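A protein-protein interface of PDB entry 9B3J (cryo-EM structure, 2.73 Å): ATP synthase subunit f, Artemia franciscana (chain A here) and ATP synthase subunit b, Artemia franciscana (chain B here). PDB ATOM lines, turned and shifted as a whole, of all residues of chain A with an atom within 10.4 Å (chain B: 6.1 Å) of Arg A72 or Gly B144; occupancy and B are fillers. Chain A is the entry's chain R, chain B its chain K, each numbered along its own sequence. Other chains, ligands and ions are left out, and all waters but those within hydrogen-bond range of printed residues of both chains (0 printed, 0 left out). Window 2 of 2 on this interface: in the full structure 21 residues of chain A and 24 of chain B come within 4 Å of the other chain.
NE of Arg B62 lies within hydrogen-bond range of O of Leu A70 (2.9 Å). N of Lys A73 lies within hydrogen-bond range of O of Val B64, 3.2 Å away. The guanidinium group (NE) of Arg A72 is in salt-bridge range of the side-chain carboxylate (OD1) of Asp B140, 3.6 Å away.
The backbone NH (N) of Leu A70 sits at hydrogen-bond distance from the backbone carbonyl oxygen (O) of Gln A65 (2.7 Å).
Among the printed residues, pairs that only touch across the chains: Lys A73 with Asp B140, Pro A71 with Pro B63, Arg A72 with Ile B143, Arg A72 with Pro B63, Arg A72 with Arg B62 and Arg A72 with Gly B144.
Arg A72 touches five residues of chain B. Of chain A, only Arg A72 (3.97 Å) comes within 4 Å of Gly B144. Of the printed residues of chain A, Asp B140 touches Arg A72 (3.6 Å) and Lys A73 (3.3 Å). Of the printed residues of chain A, Pro B63 touches Pro A71 (3.4 Å) and Arg A72 (3.6 Å). Of the printed residues of chain B, Pro A71 touches Pro B63 (3.4 Å). Of the printed residues of chain B, Lys A73 touches Val B64 and Asp B140. Printed residues of chain A within 4 Å of Val B64: Lys A73. The nearest residue of chain B that does not touch Arg A72 is Val B64 (4.2 Å).
Printed residues of chain B that touch a printed residue of chain A: Arg B62, Pro B63, Val B64, Asp B140, Ile B143 and Gly B144. Of the 13 printed residues of chain A, 4 touch a printed residue of chain B. Printed residues of chain A that touch a printed residue of chain B: Leu A70, Pro A71, Arg A72 and Lys A73. Hydrophobic or aromatic side chains of chain A within 4 Å of the printed part of chain B: Pro A71. Along chain A the printed residues that touch a printed residue of chain B span positions 70 to 73.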
ATOM      1  N   GLN A  65       4.670   0.305   8.764  1.00  0.00           N
ATOM      2  CA  GLN A  65       4.967  -0.890   9.541  1.00  0.00           C
ATOM      3  C   GLN A  65       5.915  -0.566  10.684  1.00  0.00           C
ATOM      4  O   GLN A  65       5.727  -1.035  11.811  1.00  0.00           O
ATOM      5  CB  GLN A  65       5.557  -1.971   8.642  1.00  0.00           C
ATOM      6  CG  GLN A  65       4.563  -2.643   7.725  1.00  0.00           C
ATOM      7  CD  GLN A  65       3.828  -3.774   8.386  1.00  0.00           C
ATOM      8  OE1 GLN A  65       4.169  -4.183   9.484  1.00  0.00           O
ATOM      9  NE2 GLN A  65       2.815  -4.295   7.716  1.00  0.00           N
ATOM     10  N   HIS A  66       6.922   0.265  10.417  1.00  0.00           N
ATOM     11  CA  HIS A  66       7.879   0.647  11.440  1.00  0.00           C
ATOM     12  C   HIS A  66       7.270   1.531  12.511  1.00  0.00           C
ATOM     13  O   HIS A  66       7.802   1.586  13.622  1.00  0.00           O
ATOM     14  CB  HIS A  66       9.060   1.369  10.807  1.00  0.00           C
ATOM     15  CG  HIS A  66      10.260   0.500  10.623  1.00  0.00           C
ATOM     16  ND1 HIS A  66      10.864  -0.156  11.672  1.00  0.00           N
ATOM     17  CD2 HIS A  66      10.970   0.181   9.518  1.00  0.00           C
ATOM     18  CE1 HIS A  66      11.897  -0.841  11.219  1.00  0.00           C
ATOM     19  NE2 HIS A  66      11.982  -0.653   9.915  1.00  0.00           N
ATOM     20  N   LYS A  67       6.195   2.245  12.207  1.00  0.00           N
ATOM     21  CA  LYS A  67       5.619   3.122  13.211  1.00  0.00           C
ATOM     22  C   LYS A  67       4.562   2.439  14.058  1.00  0.00           C
ATOM     23  O   LYS A  67       4.457   2.742  15.249  1.00  0.00           O
ATOM     24  CB  LYS A  67       5.023   4.359  12.541  1.00  0.00           C
ATOM     25  CG  LYS A  67       4.663   5.479  13.482  1.00  0.00           C
ATOM     26  CD  LYS A  67       4.372   6.741  12.700  1.00  0.00           C
ATOM     27  CE  LYS A  67       3.999   7.886  13.612  1.00  0.00           C
ATOM     28  NZ  LYS A  67       2.683   7.667  14.261  1.00  0.00           N
ATOM     29  N   TYR A  68       3.785   1.513  13.490  1.00  0.00           N
ATOM     30  CA  TYR A  68       2.625   0.987  14.195  1.00  0.00           C
ATOM     31  C   TYR A  68       2.627  -0.511  14.440  1.00  0.00           C
ATOM     32  O   TYR A  68       1.810  -0.975  15.240  1.00  0.00           O
ATOM     33  CB  TYR A  68       1.336   1.326  13.440  1.00  0.00           C
ATOM     34  CG  TYR A  68       1.017   2.784  13.413  1.00  0.00           C
ATOM     35  CD1 TYR A  68       1.535   3.598  12.429  1.00  0.00           C
ATOM     36  CD2 TYR A  68       0.193   3.348  14.362  1.00  0.00           C
ATOM     37  CE1 TYR A  68       1.252   4.930  12.395  1.00  0.00           C
ATOM     38  CE2 TYR A  68      -0.098   4.682  14.333  1.00  0.00           C
ATOM     39  CZ  TYR A  68       0.437   5.466  13.346  1.00  0.00           C
ATOM     40  OH  TYR A  68       0.163   6.801  13.302  1.00  0.00           O
ATOM     41  N   VAL A  69       3.476  -1.291  13.774  1.00  0.00           N
ATOM     42  CA  VAL A  69       3.450  -2.744  13.891  1.00  0.00           C
ATOM     43  C   VAL A  69       4.781  -3.298  14.390  1.00  0.00           C
ATOM     44  O   VAL A  69       4.820  -4.079  15.345  1.00  0.00           O
ATOM     45  CB  VAL A  69       3.046  -3.409  12.560  1.00  0.00           C
ATOM     46  CG1 VAL A  69       3.063  -4.909  12.705  1.00  0.00           C
ATOM     47  CG2 VAL A  69       1.670  -2.970  12.156  1.00  0.00           C
ATOM     48  N   LEU A  70       5.881  -2.914  13.747  1.00  0.00           N
ATOM     49  CA  LEU A  70       7.186  -3.461  14.111  1.00  0.00           C
ATOM     50  C   LEU A  70       7.679  -3.158  15.530  1.00  0.00           C
ATOM     51  O   LEU A  70       8.517  -3.936  16.016  1.00  0.00           O
ATOM     52  CB  LEU A  70       8.235  -2.996  13.092  1.00  0.00           C
ATOM     53  CG  LEU A  70       8.063  -3.543  11.678  1.00  0.00           C
ATOM     54  CD1 LEU A  70       9.153  -3.012  10.781  1.00  0.00           C
ATOM     55  CD2 LEU A  70       8.067  -5.049  11.693  1.00  0.00           C
ATOM     56  N   PRO A  71       7.281  -2.081  16.218  1.00  0.00           N
ATOM     57  CA  PRO A  71       7.617  -1.978  17.640  1.00  0.00           C
ATOM     58  C   PRO A  71       7.035  -3.118  18.457  1.00  0.00           C
ATOM     59  O   PRO A  71       6.012  -3.706  18.103  1.00  0.00           O
ATOM     60  CB  PRO A  71       7.011  -0.639  18.040  1.00  0.00           C
ATOM     61  CG  PRO A  71       7.224   0.164  16.866  1.00  0.00           C
ATOM     62  CD  PRO A  71       6.982  -0.737  15.693  1.00  0.00           C
ATOM     63  N   ARG A  72       7.730  -3.433  19.556  1.00  0.00           N
ATOM     64  CA  ARG A  72       7.460  -4.655  20.305  1.00  0.00           C
ATOM     65  C   ARG A  72       6.070  -4.643  20.920  1.00  0.00           C
ATOM     66  O   ARG A  72       5.283  -5.572  20.717  1.00  0.00           O
ATOM     67  CB  ARG A  72       8.515  -4.844  21.390  1.00  0.00           C
ATOM     68  CG  ARG A  72       8.387  -6.151  22.147  1.00  0.00           C
ATOM     69  CD  ARG A  72       9.337  -6.175  23.328  1.00  0.00           C
ATOM     70  NE  ARG A  72       9.109  -7.316  24.205  1.00  0.00           N
ATOM     71  CZ  ARG A  72       9.578  -7.414  25.441  1.00  0.00           C
ATOM     72  NH1 ARG A  72      10.290  -6.444  25.988  1.00  0.00           N
ATOM     73  NH2 ARG A  72       9.324  -8.512  26.147  1.00  0.00           N
ATOM     74  N   LYS A  73       5.741  -3.595  21.662  1.00  0.00           N
ATOM     75  CA  LYS A  73       4.428  -3.526  22.294  1.00  0.00           C
ATOM     76  C   LYS A  73       3.429  -2.778  21.425  1.00  0.00           C
ATOM     77  O   LYS A  73       2.783  -1.833  21.862  1.00  0.00           O
ATOM     78  CB  LYS A  73       4.548  -2.892  23.672  1.00  0.00           C
ATOM     79  CG  LYS A  73       5.417  -3.697  24.620  1.00  0.00           C
ATOM     80  CD  LYS A  73       5.294  -3.210  26.050  1.00  0.00           C
ATOM     81  CE  LYS A  73       6.048  -4.121  26.999  1.00  0.00           C
ATOM     82  NZ  LYS A  73       5.817  -3.743  28.418  1.00  0.00           N
ATOM     83  N   GLY A  74       3.292  -3.215  20.177  1.00  0.00           N
ATOM     84  CA  GLY A  74       2.345  -2.594  19.279  1.00  0.00           C
ATOM     85  C   GLY A  74       0.911  -2.935  19.627  1.00  0.00           C
ATOM     86  O   GLY A  74       0.615  -3.921  20.300  1.00  0.00           O
ATOM     87  N   GLY A  75      -0.001  -2.090  19.152  1.00  0.00           N
ATOM     88  CA  GLY A  75      -1.398  -2.187  19.491  1.00  0.00           C
ATOM     89  C   GLY A  75      -2.265  -2.618  18.326  1.00  0.00           C
ATOM     90  O   GLY A  75      -1.785  -3.087  17.292  1.00  0.00           O
ATOM     91  N   ILE A  76      -3.579  -2.460  18.517  1.00  0.00           N
ATOM     92  CA  ILE A  76      -4.540  -2.774  17.470  1.00  0.00           C
ATOM     93  C   ILE A  76      -4.900  -1.547  16.651  1.00  0.00           C
ATOM     94  O   ILE A  76      -5.697  -1.647  15.709  1.00  0.00           O
ATOM     95  CB  ILE A  76      -5.794  -3.435  18.079  1.00  0.00           C
ATOM     96  CG1 ILE A  76      -6.448  -4.382  17.068  1.00  0.00           C
ATOM     97  CG2 ILE A  76      -6.764  -2.391  18.610  1.00  0.00           C
ATOM     98  CD1 ILE A  76      -7.770  -4.936  17.506  1.00  0.00           C
ATOM     99  N   PRO A  78      -2.967  -0.111  14.304  1.00  0.00           N
ATOM    100  CA  PRO A  78      -2.718  -0.364  12.878  1.00  0.00           C
ATOM    101  C   PRO A  78      -3.784  -1.189  12.199  1.00  0.00           C
ATOM    102  O   PRO A  78      -4.089  -0.946  11.026  1.00  0.00           O
ATOM    103  CB  PRO A  78      -1.378  -1.100  12.888  1.00  0.00           C
ATOM    104  CG  PRO A  78      -1.257  -1.644  14.217  1.00  0.00           C
ATOM    105  CD  PRO A  78      -1.814  -0.588  15.087  1.00  0.00           C
ATOM    106  N   ARG B  62      14.490  -0.214  17.691  1.00  0.00           N
ATOM    107  CA  ARG B  62      13.147  -0.718  17.918  1.00  0.00           C
ATOM    108  C   ARG B  62      12.555  -0.038  19.136  1.00  0.00           C
ATOM    109  O   ARG B  62      12.962  -0.351  20.265  1.00  0.00           O
ATOM    110  CB  ARG B  62      13.170  -2.229  18.116  1.00  0.00           C
ATOM    111  CG  ARG B  62      11.803  -2.848  18.126  1.00  0.00           C
ATOM    112  CD  ARG B  62      11.901  -4.342  18.135  1.00  0.00           C
ATOM    113  NE  ARG B  62      10.661  -4.951  17.686  1.00  0.00           N
ATOM    114  CZ  ARG B  62      10.393  -6.241  17.802  1.00  0.00           C
ATOM    115  NH1 ARG B  62      11.260  -7.075  18.341  1.00  0.00           N
ATOM    116  NH2 ARG B  62       9.224  -6.701  17.377  1.00  0.00           N
ATOM    117  N   PRO B  63      11.619   0.892  18.978  1.00  0.00           N
ATOM    118  CA  PRO B  63      10.997   1.509  20.148  1.00  0.00           C
ATOM    119  C   PRO B  63      10.079   0.541  20.872  1.00  0.00           C
ATOM    120  O   PRO B  63       9.539  -0.401  20.288  1.00  0.00           O
ATOM    121  CB  PRO B  63      10.214   2.682  19.553  1.00  0.00           C
ATOM    122  CG  PRO B  63       9.929   2.263  18.174  1.00  0.00           C
ATOM    123  CD  PRO B  63      11.124   1.482  17.726  1.00  0.00           C
ATOM    124  N   VAL B  64       9.925   0.778  22.174  1.00  0.00           N
ATOM    125  CA  VAL B  64       9.053  -0.057  22.988  1.00  0.00           C
ATOM    126  C   VAL B  64       7.594   0.199  22.644  1.00  0.00           C
ATOM    127  O   VAL B  64       6.786  -0.732  22.574  1.00  0.00           O
ATOM    128  CB  VAL B  64       9.325   0.190  24.481  1.00  0.00           C
ATOM    129  CG1 VAL B  64       8.658  -0.889  25.329  1.00  0.00           C
ATOM    130  CG2 VAL B  64      10.817   0.264  24.745  1.00  0.00           C
ATOM    131  N   ASN B  65       7.238   1.449  22.434  1.00  0.00           N
ATOM    132  CA  ASN B  65       5.860   1.824  22.208  1.00  0.00           C
ATOM    133  C   ASN B  65       5.663   2.345  20.794  1.00  0.00           C
ATOM    134  O   ASN B  65       6.497   3.108  20.295  1.00  0.00           O
ATOM    135  CB  ASN B  65       5.421   2.904  23.199  1.00  0.00           C
ATOM    136  CG  ASN B  65       5.226   2.366  24.595  1.00  0.00           C
ATOM    137  OD1 ASN B  65       4.700   1.270  24.781  1.00  0.00           O
ATOM    138  ND2 ASN B  65       5.650   3.135  25.589  1.00  0.00           N
ATOM    139  N   ALA B 139       1.193 -12.334  24.467  1.00  0.00           N
ATOM    140  CA  ALA B 139       2.210 -12.096  23.452  1.00  0.00           C
ATOM    141  C   ALA B 139       3.532 -11.666  24.074  1.00  0.00           C
ATOM    142  O   ALA B 139       4.596 -12.156  23.674  1.00  0.00           O
ATOM    143  CB  ALA B 139       1.720 -11.052  22.455  1.00  0.00           C
ATOM    144  N   ASP B 140       3.495 -10.766  25.061  1.00  0.00           N
ATOM    145  CA  ASP B 140       4.737 -10.308  25.671  1.00  0.00           C
ATOM    146  C   ASP B 140       5.381 -11.387  26.525  1.00  0.00           C
ATOM    147  O   ASP B 140       6.605 -11.384  26.703  1.00  0.00           O
ATOM    148  CB  ASP B 140       4.490  -9.056  26.500  1.00  0.00           C
ATOM    149  CG  ASP B 140       4.773  -7.793  25.730  1.00  0.00           C
ATOM    150  OD1 ASP B 140       5.544  -7.860  24.753  1.00  0.00           O
ATOM    151  OD2 ASP B 140       4.231  -6.732  26.101  1.00  0.00           O
ATOM    152  N   LYS B 141       4.583 -12.321  27.047  1.00  0.00           N
ATOM    153  CA  LYS B 141       5.143 -13.490  27.710  1.00  0.00           C
ATOM    154  C   LYS B 141       5.924 -14.345  26.726  1.00  0.00           C
ATOM    155  O   LYS B 141       7.027 -14.817  27.040  1.00  0.00           O
ATOM    156  CB  LYS B 141       4.019 -14.297  28.356  1.00  0.00           C
ATOM    157  CG  LYS B 141       4.408 -15.682  28.817  1.00  0.00           C
ATOM    158  CD  LYS B 141       3.178 -16.458  29.251  1.00  0.00           C
ATOM    159  CE  LYS B 141       3.531 -17.880  29.640  1.00  0.00           C
ATOM    160  NZ  LYS B 141       2.326 -18.660  30.024  1.00  0.00           N
ATOM    161  N   GLY B 142       5.380 -14.536  25.522  1.00  0.00           N
ATOM    162  CA  GLY B 142       6.107 -15.297  24.513  1.00  0.00           C
ATOM    163  C   GLY B 142       7.384 -14.620  24.044  1.00  0.00           C
ATOM    164  O   GLY B 142       8.411 -15.280  23.842  1.00  0.00           O
ATOM    165  N   ILE B 143       7.340 -13.298  23.857  1.00  0.00           N
ATOM    166  CA  ILE B 143       8.527 -12.572  23.405  1.00  0.00           C
ATOM    167  C   ILE B 143       9.597 -12.575  24.489  1.00  0.00           C
ATOM    168  O   ILE B 143      10.797 -12.686  24.201  1.00  0.00           O
ATOM    169  CB  ILE B 143       8.168 -11.134  22.984  1.00  0.00           C
ATOM    170  CG1 ILE B 143       7.052 -11.120  21.946  1.00  0.00           C
ATOM    171  CG2 ILE B 143       9.375 -10.412  22.428  1.00  0.00           C
ATOM    172  CD1 ILE B 143       7.259 -12.047  20.817  1.00  0.00           C
ATOM    173  N   GLY B 144       9.183 -12.461  25.753  1.00  0.00           N
ATOM    174  CA  GLY B 144      10.136 -12.574  26.841  1.00  0.00           C
ATOM    175  C   GLY B 144      10.759 -13.952  26.936  1.00  0.00           C
ATOM    176  O   GLY B 144      11.947 -14.079  27.223  1.00  0.00           O
ATOM    177  N   GLU B 145       9.966 -15.002  26.691  1.00  0.00           N
ATOM    178  CA  GLU B 145      10.509 -16.359  26.698  1.00  0.00           C
ATOM    179  C   GLU B 145      11.526 -16.559  25.584  1.00  0.00           C
ATOM    180  O   GLU B 145      12.555 -17.217  25.784  1.00  0.00           O
ATOM    181  CB  GLU B 145       9.383 -17.380  26.569  1.00  0.00           C
ATOM    182  CG  GLU B 145       8.572 -17.574  27.834  1.00  0.00           C
ATOM    183  CD  GLU B 145       7.479 -18.612  27.674  1.00  0.00           C
ATOM    184  OE1 GLU B 145       7.463 -19.311  26.638  1.00  0.00           O
ATOM    185  OE2 GLU B 145       6.632 -18.731  28.584  1.00  0.00           O
ATOM    186  N   ILE B 146      11.258 -15.996  24.406  1.00  0.00           N
ATOM    187  CA  ILE B 146      12.203 -16.112  23.296  1.00  0.00           C
ATOM    188  C   ILE B 146      13.490 -15.352  23.599  1.00  0.00           C
ATOM    189  O   ILE B 146      14.600 -15.869  23.403  1.00  0.00           O
ATOM    190  CB  ILE B 146      11.554 -15.628  21.990  1.00  0.00           C
ATOM    191  CG1 ILE B 146      10.453 -16.593  21.561  1.00  0.00           C
ATOM    192  CG2 ILE B 146      12.585 -15.506  20.897  1.00  0.00           C
ATOM    193  CD1 ILE B 146       9.751 -16.185  20.299  1.00  0.00           C
ATOM    194  N   GLU B 147      13.364 -14.117  24.092  1.00  0.00           N
ATOM    195  CA  GLU B 147      14.548 -13.327  24.416  1.00  0.00           C
ATOM    196  C   GLU B 147      15.333 -13.940  25.568  1.00  0.00           C
ATOM    197  O   GLU B 147      16.570 -13.889  25.577  1.00  0.00           O
ATOM    198  CB  GLU B 147      14.135 -11.895  24.741  1.00  0.00           C
ATOM    199  CG  GLU B 147      15.284 -10.943  24.979  1.00  0.00           C
ATOM    200  CD  GLU B 147      14.815  -9.514  25.173  1.00  0.00           C
ATOM    201  OE1 GLU B 147      13.857  -9.105  24.488  1.00  0.00           O
ATOM    202  OE2 GLU B 147      15.397  -8.803  26.018  1.00  0.00           O
ATOM    203  N   GLN B 148      14.636 -14.544  26.532  1.00  0.00           N
ATOM    204  CA  GLN B 148      15.301 -15.251  27.618  1.00  0.00           C
ATOM    205  C   GLN B 148      16.061 -16.458  27.098  1.00  0.00           C
ATOM    206  O   GLN B 148      17.174 -16.736  27.553  1.00  0.00           O
ATOM    207  CB  GLN B 148      14.274 -15.674  28.666  1.00  0.00           C
ATOM    208  CG  GLN B 148      14.832 -16.473  29.826  1.00  0.00           C
ATOM    209  CD  GLN B 148      13.759 -16.839  30.828  1.00  0.00           C
ATOM    210  OE1 GLN B 148      12.665 -16.277  30.812  1.00  0.00           O
ATOM    211  NE2 GLN B 148      14.064 -17.789  31.705  1.00  0.00           N
ATOM    212  N   SER B 149      15.479 -17.182  26.138  1.00  0.00           N
ATOM    213  CA  SER B 149      16.166 -18.337  25.571  1.00  0.00           C
ATOM    214  C   SER B 149      17.408 -17.920  24.792  1.00  0.00           C
ATOM    215  O   SER B 149      18.433 -18.614  24.831  1.00  0.00           O
ATOM    216  CB  SER B 149      15.212 -19.123  24.678  1.00  0.00           C
ATOM    217  OG  SER B 149      14.842 -18.361  23.547  1.00  0.00           O
